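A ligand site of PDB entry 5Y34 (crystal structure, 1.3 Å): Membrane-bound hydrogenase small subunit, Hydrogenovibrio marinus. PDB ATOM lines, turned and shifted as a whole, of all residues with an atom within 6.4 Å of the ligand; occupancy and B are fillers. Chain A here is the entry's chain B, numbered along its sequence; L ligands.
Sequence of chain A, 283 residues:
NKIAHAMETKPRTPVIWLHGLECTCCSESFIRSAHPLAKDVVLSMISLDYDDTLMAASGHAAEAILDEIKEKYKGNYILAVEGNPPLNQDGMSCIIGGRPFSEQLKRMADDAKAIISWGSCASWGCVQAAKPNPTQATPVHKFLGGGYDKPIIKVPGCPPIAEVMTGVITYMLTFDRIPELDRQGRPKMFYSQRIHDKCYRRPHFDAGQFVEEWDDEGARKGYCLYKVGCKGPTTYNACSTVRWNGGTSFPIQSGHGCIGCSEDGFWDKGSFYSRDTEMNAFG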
ATOM      1  N   ILE A 195       9.246  31.308   6.405  1.00  0.00           N
ATOM      2  CA  ILE A 195      10.328  30.370   6.724  1.00  0.00           C
ATOM      3  C   ILE A 195      11.645  30.892   6.140  1.00  0.00           C
ATOM      4  O   ILE A 195      12.671  30.943   6.823  1.00  0.00           O
ATOM      5  CB  ILE A 195      10.029  28.956   6.172  1.00  0.00           C
ATOM      6  CG1 ILE A 195       8.661  28.421   6.647  1.00  0.00           C
ATOM      7  CG2 ILE A 195      11.145  27.988   6.528  1.00  0.00           C
ATOM      8  CD1 ILE A 195       8.531  28.236   8.147  1.00  0.00           C
ATOM      9  N   HIS A 196      11.595  31.298   4.864  1.00  0.00           N
ATOM     10  CA  HIS A 196      12.754  31.721   4.095  1.00  0.00           C
ATOM     11  C   HIS A 196      13.324  33.064   4.593  1.00  0.00           C
ATOM     12  O   HIS A 196      14.480  33.368   4.317  1.00  0.00           O
ATOM     13  CB  HIS A 196      12.285  31.792   2.631  1.00  0.00           C
ATOM     14  CG  HIS A 196      13.296  32.208   1.610  1.00  0.00           C
ATOM     15  ND1 HIS A 196      14.230  31.357   1.053  1.00  0.00           N
ATOM     16  CD2 HIS A 196      13.421  33.393   0.946  1.00  0.00           C
ATOM     17  CE1 HIS A 196      14.924  32.008   0.122  1.00  0.00           C
ATOM     18  NE2 HIS A 196      14.462  33.244   0.059  1.00  0.00           N
ATOM     19  N   ASP A 197      12.522  33.818   5.373  1.00  0.00           N
ATOM     20  CA  ASP A 197      12.938  35.071   6.035  1.00  0.00           C
ATOM     21  C   ASP A 197      13.803  34.847   7.274  1.00  0.00           C
ATOM     22  O   ASP A 197      14.319  35.818   7.826  1.00  0.00           O
ATOM     23  CB  ASP A 197      11.730  35.903   6.543  1.00  0.00           C
ATOM     24  CG  ASP A 197      10.794  36.391   5.458  1.00  0.00           C
ATOM     25  OD1 ASP A 197      11.207  36.625   4.309  1.00  0.00           O
ATOM     26  OD2 ASP A 197       9.599  36.609   5.806  1.00  0.00           O
ATOM     27  N   CYS A 199      15.673  31.518   7.586  1.00  0.00           N
ATOM     28  CA  CYS A 199      16.235  30.207   7.301  1.00  0.00           C
ATOM     29  C   CYS A 199      17.738  30.140   7.334  1.00  0.00           C
ATOM     30  O   CYS A 199      18.426  30.850   6.596  1.00  0.00           O
ATOM     31  CB  CYS A 199      15.680  29.627   5.981  1.00  0.00           C
ATOM     32  SG  CYS A 199      16.257  27.940   5.637  1.00  0.00           S
ATOM     33  N   TYR A 200      18.269  29.242   8.153  1.00  0.00           N
ATOM     34  CA  TYR A 200      19.718  29.099   8.320  1.00  0.00           C
ATOM     35  C   TYR A 200      20.431  28.622   7.030  1.00  0.00           C
ATOM     36  O   TYR A 200      21.649  28.754   6.919  1.00  0.00           O
ATOM     37  CB  TYR A 200      20.035  28.186   9.535  1.00  0.00           C
ATOM     38  CG  TYR A 200      19.985  26.737   9.189  1.00  0.00           C
ATOM     39  CD1 TYR A 200      18.768  26.099   8.915  1.00  0.00           C
ATOM     40  CD2 TYR A 200      21.161  25.987   9.088  1.00  0.00           C
ATOM     41  CE1 TYR A 200      18.706  24.772   8.542  1.00  0.00           C
ATOM     42  CE2 TYR A 200      21.114  24.641   8.730  1.00  0.00           C
ATOM     43  CZ  TYR A 200      19.889  24.038   8.468  1.00  0.00           C
ATOM     44  OH  TYR A 200      19.825  22.737   8.063  1.00  0.00           O
ATOM     45  N   ARG A 201      19.670  28.052   6.088  1.00  0.00           N
ATOM     46  CA  ARG A 201      20.255  27.669   4.775  1.00  0.00           C
ATOM     47  C   ARG A 201      20.234  28.832   3.760  1.00  0.00           C
ATOM     48  O   ARG A 201      20.755  28.672   2.648  1.00  0.00           O
ATOM     49  CB  ARG A 201      19.611  26.426   4.171  1.00  0.00           C
ATOM     50  CG  ARG A 201      19.728  25.184   5.074  1.00  0.00           C
ATOM     51  CD  ARG A 201      19.354  23.943   4.279  1.00  0.00           C
ATOM     52  NE  ARG A 201      19.436  22.728   5.132  1.00  0.00           N
ATOM     53  CZ  ARG A 201      19.604  21.491   4.675  1.00  0.00           C
ATOM     54  NH1 ARG A 201      19.652  20.479   5.542  1.00  0.00           N
ATOM     55  NH2 ARG A 201      19.737  21.206   3.384  1.00  0.00           N
ATOM     56  N   ARG A 202      19.708  29.989   4.167  1.00  0.00           N
ATOM     57  CA  ARG A 202      19.671  31.157   3.252  1.00  0.00           C
ATOM     58  C   ARG A 202      21.035  31.542   2.666  1.00  0.00           C
ATOM     59  O   ARG A 202      21.098  31.899   1.479  1.00  0.00           O
ATOM     60  CB  ARG A 202      19.011  32.360   3.928  1.00  0.00           C
ATOM     61  CG  ARG A 202      18.953  33.590   3.029  1.00  0.00           C
ATOM     62  CD  ARG A 202      17.880  33.441   1.961  1.00  0.00           C
ATOM     63  NE  ARG A 202      17.795  34.725   1.273  1.00  0.00           N
ATOM     64  CZ  ARG A 202      16.831  35.615   1.499  1.00  0.00           C
ATOM     65  NH1 ARG A 202      15.821  35.344   2.311  1.00  0.00           N
ATOM     66  NH2 ARG A 202      16.844  36.777   0.881  1.00  0.00           N
ATOM     67  N   PRO A 203      22.137  31.467   3.436  1.00  0.00           N
ATOM     68  CA  PRO A 203      23.441  31.775   2.805  1.00  0.00           C
ATOM     69  C   PRO A 203      23.705  30.953   1.552  1.00  0.00           C
ATOM     70  O   PRO A 203      24.287  31.469   0.573  1.00  0.00           O
ATOM     71  CB  PRO A 203      24.452  31.437   3.904  1.00  0.00           C
ATOM     72  CG  PRO A 203      23.677  31.675   5.168  1.00  0.00           C
ATOM     73  CD  PRO A 203      22.284  31.171   4.878  1.00  0.00           C
ATOM     74  N   PHE A 205      21.270  29.575  -0.496  1.00  0.00           N
ATOM     75  CA  PHE A 205      20.348  30.125  -1.482  1.00  0.00           C
ATOM     76  C   PHE A 205      21.012  31.335  -2.147  1.00  0.00           C
ATOM     77  O   PHE A 205      21.044  31.460  -3.398  1.00  0.00           O
ATOM     78  CB  PHE A 205      19.055  30.574  -0.796  1.00  0.00           C
ATOM     79  CG  PHE A 205      18.072  31.250  -1.728  1.00  0.00           C
ATOM     80  CD1 PHE A 205      17.142  30.505  -2.446  1.00  0.00           C
ATOM     81  CD2 PHE A 205      18.033  32.637  -1.826  1.00  0.00           C
ATOM     82  CE1 PHE A 205      16.195  31.118  -3.253  1.00  0.00           C
ATOM     83  CE2 PHE A 205      17.111  33.268  -2.665  1.00  0.00           C
ATOM     84  CZ  PHE A 205      16.197  32.504  -3.367  1.00  0.00           C
ATOM     85  N   PHE A 210      22.777  24.757  -4.049  1.00  0.00           N
ATOM     86  CA  PHE A 210      21.534  24.004  -3.908  1.00  0.00           C
ATOM     87  C   PHE A 210      21.780  22.518  -3.900  1.00  0.00           C
ATOM     88  O   PHE A 210      22.725  22.005  -4.496  1.00  0.00           O
ATOM     89  CB  PHE A 210      20.601  24.302  -5.108  1.00  0.00           C
ATOM     90  CG  PHE A 210      20.228  25.738  -5.243  1.00  0.00           C
ATOM     91  CD1 PHE A 210      19.357  26.343  -4.349  1.00  0.00           C
ATOM     92  CD2 PHE A 210      20.731  26.495  -6.315  1.00  0.00           C
ATOM     93  CE1 PHE A 210      19.009  27.667  -4.473  1.00  0.00           C
ATOM     94  CE2 PHE A 210      20.377  27.834  -6.455  1.00  0.00           C
ATOM     95  CZ  PHE A 210      19.511  28.424  -5.545  1.00  0.00           C
ATOM     96  N   TYR A 223      23.023  22.369   1.805  1.00  0.00           N
ATOM     97  CA  TYR A 223      22.704  23.433   0.852  1.00  0.00           C
ATOM     98  C   TYR A 223      21.206  23.702   0.767  1.00  0.00           C
ATOM     99  O   TYR A 223      20.392  22.904   1.210  1.00  0.00           O
ATOM    100  CB  TYR A 223      23.260  23.095  -0.535  1.00  0.00           C
ATOM    101  CG  TYR A 223      24.757  23.336  -0.743  1.00  0.00           C
ATOM    102  CD1 TYR A 223      25.606  23.694   0.302  1.00  0.00           C
ATOM    103  CD2 TYR A 223      25.304  23.175  -2.014  1.00  0.00           C
ATOM    104  CE1 TYR A 223      26.976  23.909   0.085  1.00  0.00           C
ATOM    105  CE2 TYR A 223      26.659  23.379  -2.244  1.00  0.00           C
ATOM    106  CZ  TYR A 223      27.486  23.766  -1.207  1.00  0.00           C
ATOM    107  OH  TYR A 223      28.838  23.961  -1.456  1.00  0.00           O
ATOM    108  N   CYS A 224      20.833  24.818   0.168  1.00  0.00           N
ATOM    109  CA  CYS A 224      19.424  25.223   0.090  1.00  0.00           C
ATOM    110  C   CYS A 224      18.585  24.197  -0.688  1.00  0.00           C
ATOM    111  O   CYS A 224      19.066  23.573  -1.658  1.00  0.00           O
ATOM    112  CB  CYS A 224      19.368  26.588  -0.596  1.00  0.00           C
ATOM    113  SG  CYS A 224      17.712  27.137  -1.014  1.00  0.00           S
ATOM    114  N   LEU A 225      17.341  24.018  -0.227  1.00  0.00           N
ATOM    115  CA  LEU A 225      16.415  23.057  -0.799  1.00  0.00           C
ATOM    116  C   LEU A 225      15.419  23.612  -1.823  1.00  0.00           C
ATOM    117  O   LEU A 225      14.478  22.928  -2.233  1.00  0.00           O
ATOM    118  CB  LEU A 225      15.660  22.360   0.349  1.00  0.00           C
ATOM    119  CG  LEU A 225      16.558  21.617   1.352  1.00  0.00           C
ATOM    120  CD1 LEU A 225      15.795  21.188   2.620  1.00  0.00           C
ATOM    121  CD2 LEU A 225      17.197  20.414   0.671  1.00  0.00           C
ATOM    122  N   TYR A 226      15.694  24.846  -2.305  1.00  0.00           N
ATOM    123  CA  TYR A 226      14.789  25.501  -3.247  1.00  0.00           C
ATOM    124  C   TYR A 226      14.546  24.655  -4.518  1.00  0.00           C
ATOM    125  O   TYR A 226      13.399  24.509  -4.981  1.00  0.00           O
ATOM    126  CB  TYR A 226      15.341  26.883  -3.659  1.00  0.00           C
ATOM    127  CG  TYR A 226      14.447  27.490  -4.711  1.00  0.00           C
ATOM    128  CD1 TYR A 226      13.239  28.061  -4.344  1.00  0.00           C
ATOM    129  CD2 TYR A 226      14.773  27.435  -6.091  1.00  0.00           C
ATOM    130  CE1 TYR A 226      12.365  28.564  -5.279  1.00  0.00           C
ATOM    131  CE2 TYR A 226      13.882  27.920  -7.030  1.00  0.00           C
ATOM    132  CZ  TYR A 226      12.704  28.481  -6.614  1.00  0.00           C
ATOM    133  OH  TYR A 226      11.853  28.988  -7.566  1.00  0.00           O
ATOM    134  N   LYS A 227      15.622  24.087  -5.074  1.00  0.00           N
ATOM    135  CA  LYS A 227      15.496  23.360  -6.331  1.00  0.00           C
ATOM    136  C   LYS A 227      14.771  22.027  -6.213  1.00  0.00           C
ATOM    137  O   LYS A 227      14.247  21.499  -7.185  1.00  0.00           O
ATOM    138  CB  LYS A 227      16.855  23.191  -7.011  1.00  0.00           C
ATOM    139  CG  LYS A 227      17.396  24.494  -7.584  1.00  0.00           C
ATOM    140  CD  LYS A 227      18.627  24.249  -8.424  1.00  0.00           C
ATOM    141  CE  LYS A 227      18.846  25.343  -9.449  1.00  0.00           C
ATOM    142  NZ  LYS A 227      19.978  24.968 -10.332  1.00  0.00           N
ATOM    143  N   CYS A 230      11.399  23.308  -1.958  1.00  0.00           N
ATOM    144  CA  CYS A 230      11.139  24.024  -0.707  1.00  0.00           C
ATOM    145  C   CYS A 230      10.139  25.152  -0.868  1.00  0.00           C
ATOM    146  O   CYS A 230      10.341  26.028  -1.718  1.00  0.00           O
ATOM    147  CB  CYS A 230      12.431  24.572  -0.129  1.00  0.00           C
ATOM    148  SG  CYS A 230      12.145  25.262   1.526  1.00  0.00           S
ATOM    149  N   LYS A 231       9.049  25.142  -0.109  1.00  0.00           N
ATOM    150  CA  LYS A 231       8.048  26.196  -0.148  1.00  0.00           C
ATOM    151  C   LYS A 231       8.228  27.245   0.954  1.00  0.00           C
ATOM    152  O   LYS A 231       7.362  28.080   1.187  1.00  0.00           O
ATOM    153  CB  LYS A 231       6.636  25.611  -0.150  1.00  0.00           C
ATOM    154  CG  LYS A 231       6.381  24.652  -1.278  1.00  0.00           C
ATOM    155  CD  LYS A 231       6.697  25.354  -2.608  1.00  0.00           C
ATOM    156  CE  LYS A 231       6.410  24.529  -3.835  1.00  0.00           C
ATOM    157  NZ  LYS A 231       6.806  23.107  -3.810  1.00  0.00           N
ATOM    158  N   GLY A 232       9.406  27.216   1.598  1.00  0.00           N
ATOM    159  CA  GLY A 232       9.740  28.200   2.611  1.00  0.00           C
ATOM    160  C   GLY A 232       9.561  29.649   2.125  1.00  0.00           C
ATOM    161  O   GLY A 232       9.171  30.523   2.896  1.00  0.00           O
ATOM    162  N   PRO A 233       9.840  29.968   0.819  1.00  0.00           N
ATOM    163  CA  PRO A 233       9.696  31.364   0.365  1.00  0.00           C
ATOM    164  C   PRO A 233       8.290  31.943   0.452  1.00  0.00           C
ATOM    165  O   PRO A 233       8.122  33.165   0.419  1.00  0.00           O
ATOM    166  CB  PRO A 233      10.177  31.305  -1.098  1.00  0.00           C
ATOM    167  CG  PRO A 233      11.207  30.215  -1.079  1.00  0.00           C
ATOM    168  CD  PRO A 233      10.594  29.158  -0.165  1.00  0.00           C
ATOM    169  N   PHE A 250      13.624  20.997  12.126  1.00  0.00           N
ATOM    170  CA  PHE A 250      12.461  21.354  11.322  1.00  0.00           C
ATOM    171  C   PHE A 250      12.645  20.709   9.955  1.00  0.00           C
ATOM    172  O   PHE A 250      13.718  20.166   9.681  1.00  0.00           O
ATOM    173  CB  PHE A 250      12.166  22.880  11.321  1.00  0.00           C
ATOM    174  CG  PHE A 250      13.137  23.737  10.553  1.00  0.00           C
ATOM    175  CD1 PHE A 250      14.448  23.897  10.988  1.00  0.00           C
ATOM    176  CD2 PHE A 250      12.683  24.487   9.452  1.00  0.00           C
ATOM    177  CE1 PHE A 250      15.303  24.749  10.279  1.00  0.00           C
ATOM    178  CE2 PHE A 250      13.549  25.337   8.757  1.00  0.00           C
ATOM    179  CZ  PHE A 250      14.858  25.465   9.167  1.00  0.00           C
ATOM    180  N   ILE A 252      13.361  21.476   6.933  1.00  0.00           N
ATOM    181  CA  ILE A 252      14.511  21.875   6.132  1.00  0.00           C
ATOM    182  C   ILE A 252      15.813  21.413   6.788  1.00  0.00           C
ATOM    183  O   ILE A 252      16.716  20.939   6.098  1.00  0.00           O
ATOM    184  CB  ILE A 252      14.476  23.402   5.962  1.00  0.00           C
ATOM    185  CG1 ILE A 252      13.372  23.769   4.952  1.00  0.00           C
ATOM    186  CG2 ILE A 252      15.821  23.963   5.514  1.00  0.00           C
ATOM    187  CD1 ILE A 252      12.775  25.136   5.169  1.00  0.00           C
ATOM    188  N   GLY A 257      12.499  19.904   1.723  1.00  0.00           N
ATOM    189  CA  GLY A 257      11.915  21.244   1.671  1.00  0.00           C
ATOM    190  C   GLY A 257      10.601  21.350   2.440  1.00  0.00           C
ATOM    191  O   GLY A 257       9.878  20.354   2.606  1.00  0.00           O
ATOM    192  N   CYS A 258      10.322  22.536   2.961  1.00  0.00           N
ATOM    193  CA  CYS A 258       8.979  22.897   3.383  1.00  0.00           C
ATOM    194  C   CYS A 258       7.984  22.521   2.278  1.00  0.00           C
ATOM    195  O   CYS A 258       8.268  22.754   1.075  1.00  0.00           O
ATOM    196  CB  CYS A 258       8.939  24.395   3.694  1.00  0.00           C
ATOM    197  SG  CYS A 258       7.347  25.071   4.191  1.00  0.00           S
ATOM    198  N   MET A 279       9.527  34.413  -6.890  1.00  0.00           N
ATOM    199  CA  MET A 279      10.878  34.559  -6.356  1.00  0.00           C
ATOM    200  C   MET A 279      11.559  35.856  -6.789  1.00  0.00           C
ATOM    201  O   MET A 279      12.394  36.388  -6.047  1.00  0.00           O
ATOM    202  CB  MET A 279      11.726  33.352  -6.753  1.00  0.00           C
ATOM    203  CG  MET A 279      11.177  32.027  -6.198  1.00  0.00           C
ATOM    204  SD  MET A 279      10.976  31.944  -4.412  1.00  0.00           S
ATOM    205  CE  MET A 279      12.688  32.060  -3.844  1.00  0.00           C
HETATM  206 FE1  LIG L   1      15.761  27.822   3.446  1.00  0.00          FE
HETATM  207 FE2  LIG L   1      16.420  27.505   0.837  1.00  0.00          FE
HETATM  208 FE3  LIG L   1      13.935  26.767   1.695  1.00  0.00          FE
HETATM  209 FE4  LIG L   1      14.625  29.368   1.556  1.00  0.00          FE
HETATM  210  S1  LIG L   1      14.346  27.914  -0.156  1.00  0.00           S
HETATM  211  S2  LIG L   1      13.508  28.405   3.210  1.00  0.00           S
HETATM  212  S3  LIG L   1      16.820  29.286   2.161  1.00  0.00           S
HETATM  213  S4  LIG L   1      15.977  25.880   2.267  1.00  0.00           S
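The side-chain sulfur (SG) of Cys 224 binds an iron atom (FE2) of the ligand. S3 of the ligand lies close to N of Arg 202. N of Leu 225 sits close to S4 of the ligand, at 3.4 Å. FE1 of the ligand is bound by SG of Cys 199 (2.2 Å). SG of Cys 230 binds FE3 of the ligand. An iron atom (FE4) of the ligand is bound by a ring nitrogen (ND1) of His 196 (2.1 Å).
O of Ile 252 sits at hydrogen-bond distance from NH1 of Arg 201 (3.0 Å). SG of Cys 224 lies close to N of Tyr 226, 3.3 Å away. SG of Cys 230 lies close to N of Gly 232 (3.4 Å). N of Cys 258 sits close to SG of Cys 230. N of His 196 sits at hydrogen-bond distance from O of Gly 232 (3.2 Å). NE of Arg 201 sits at hydrogen-bond distance from OH of Tyr 200 (3.0 Å). NH1 of Arg 202 is in hydrogen-bond range of O of His 196 (3.1 Å). The backbone NH (N) of Arg 201 sits close to the side-chain sulfur (SG) of Cys 199 (3.4 Å).
Arg 201 touches the ligand. CB of Phe 205 touches S3 of the ligand, at 3.9 Å. Tyr 226 touches the ligand (CB to S1, 3.8 Å). Gly 232 touches the ligand. Pro 233 touches the ligand. Ile 252 touches the ligand.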
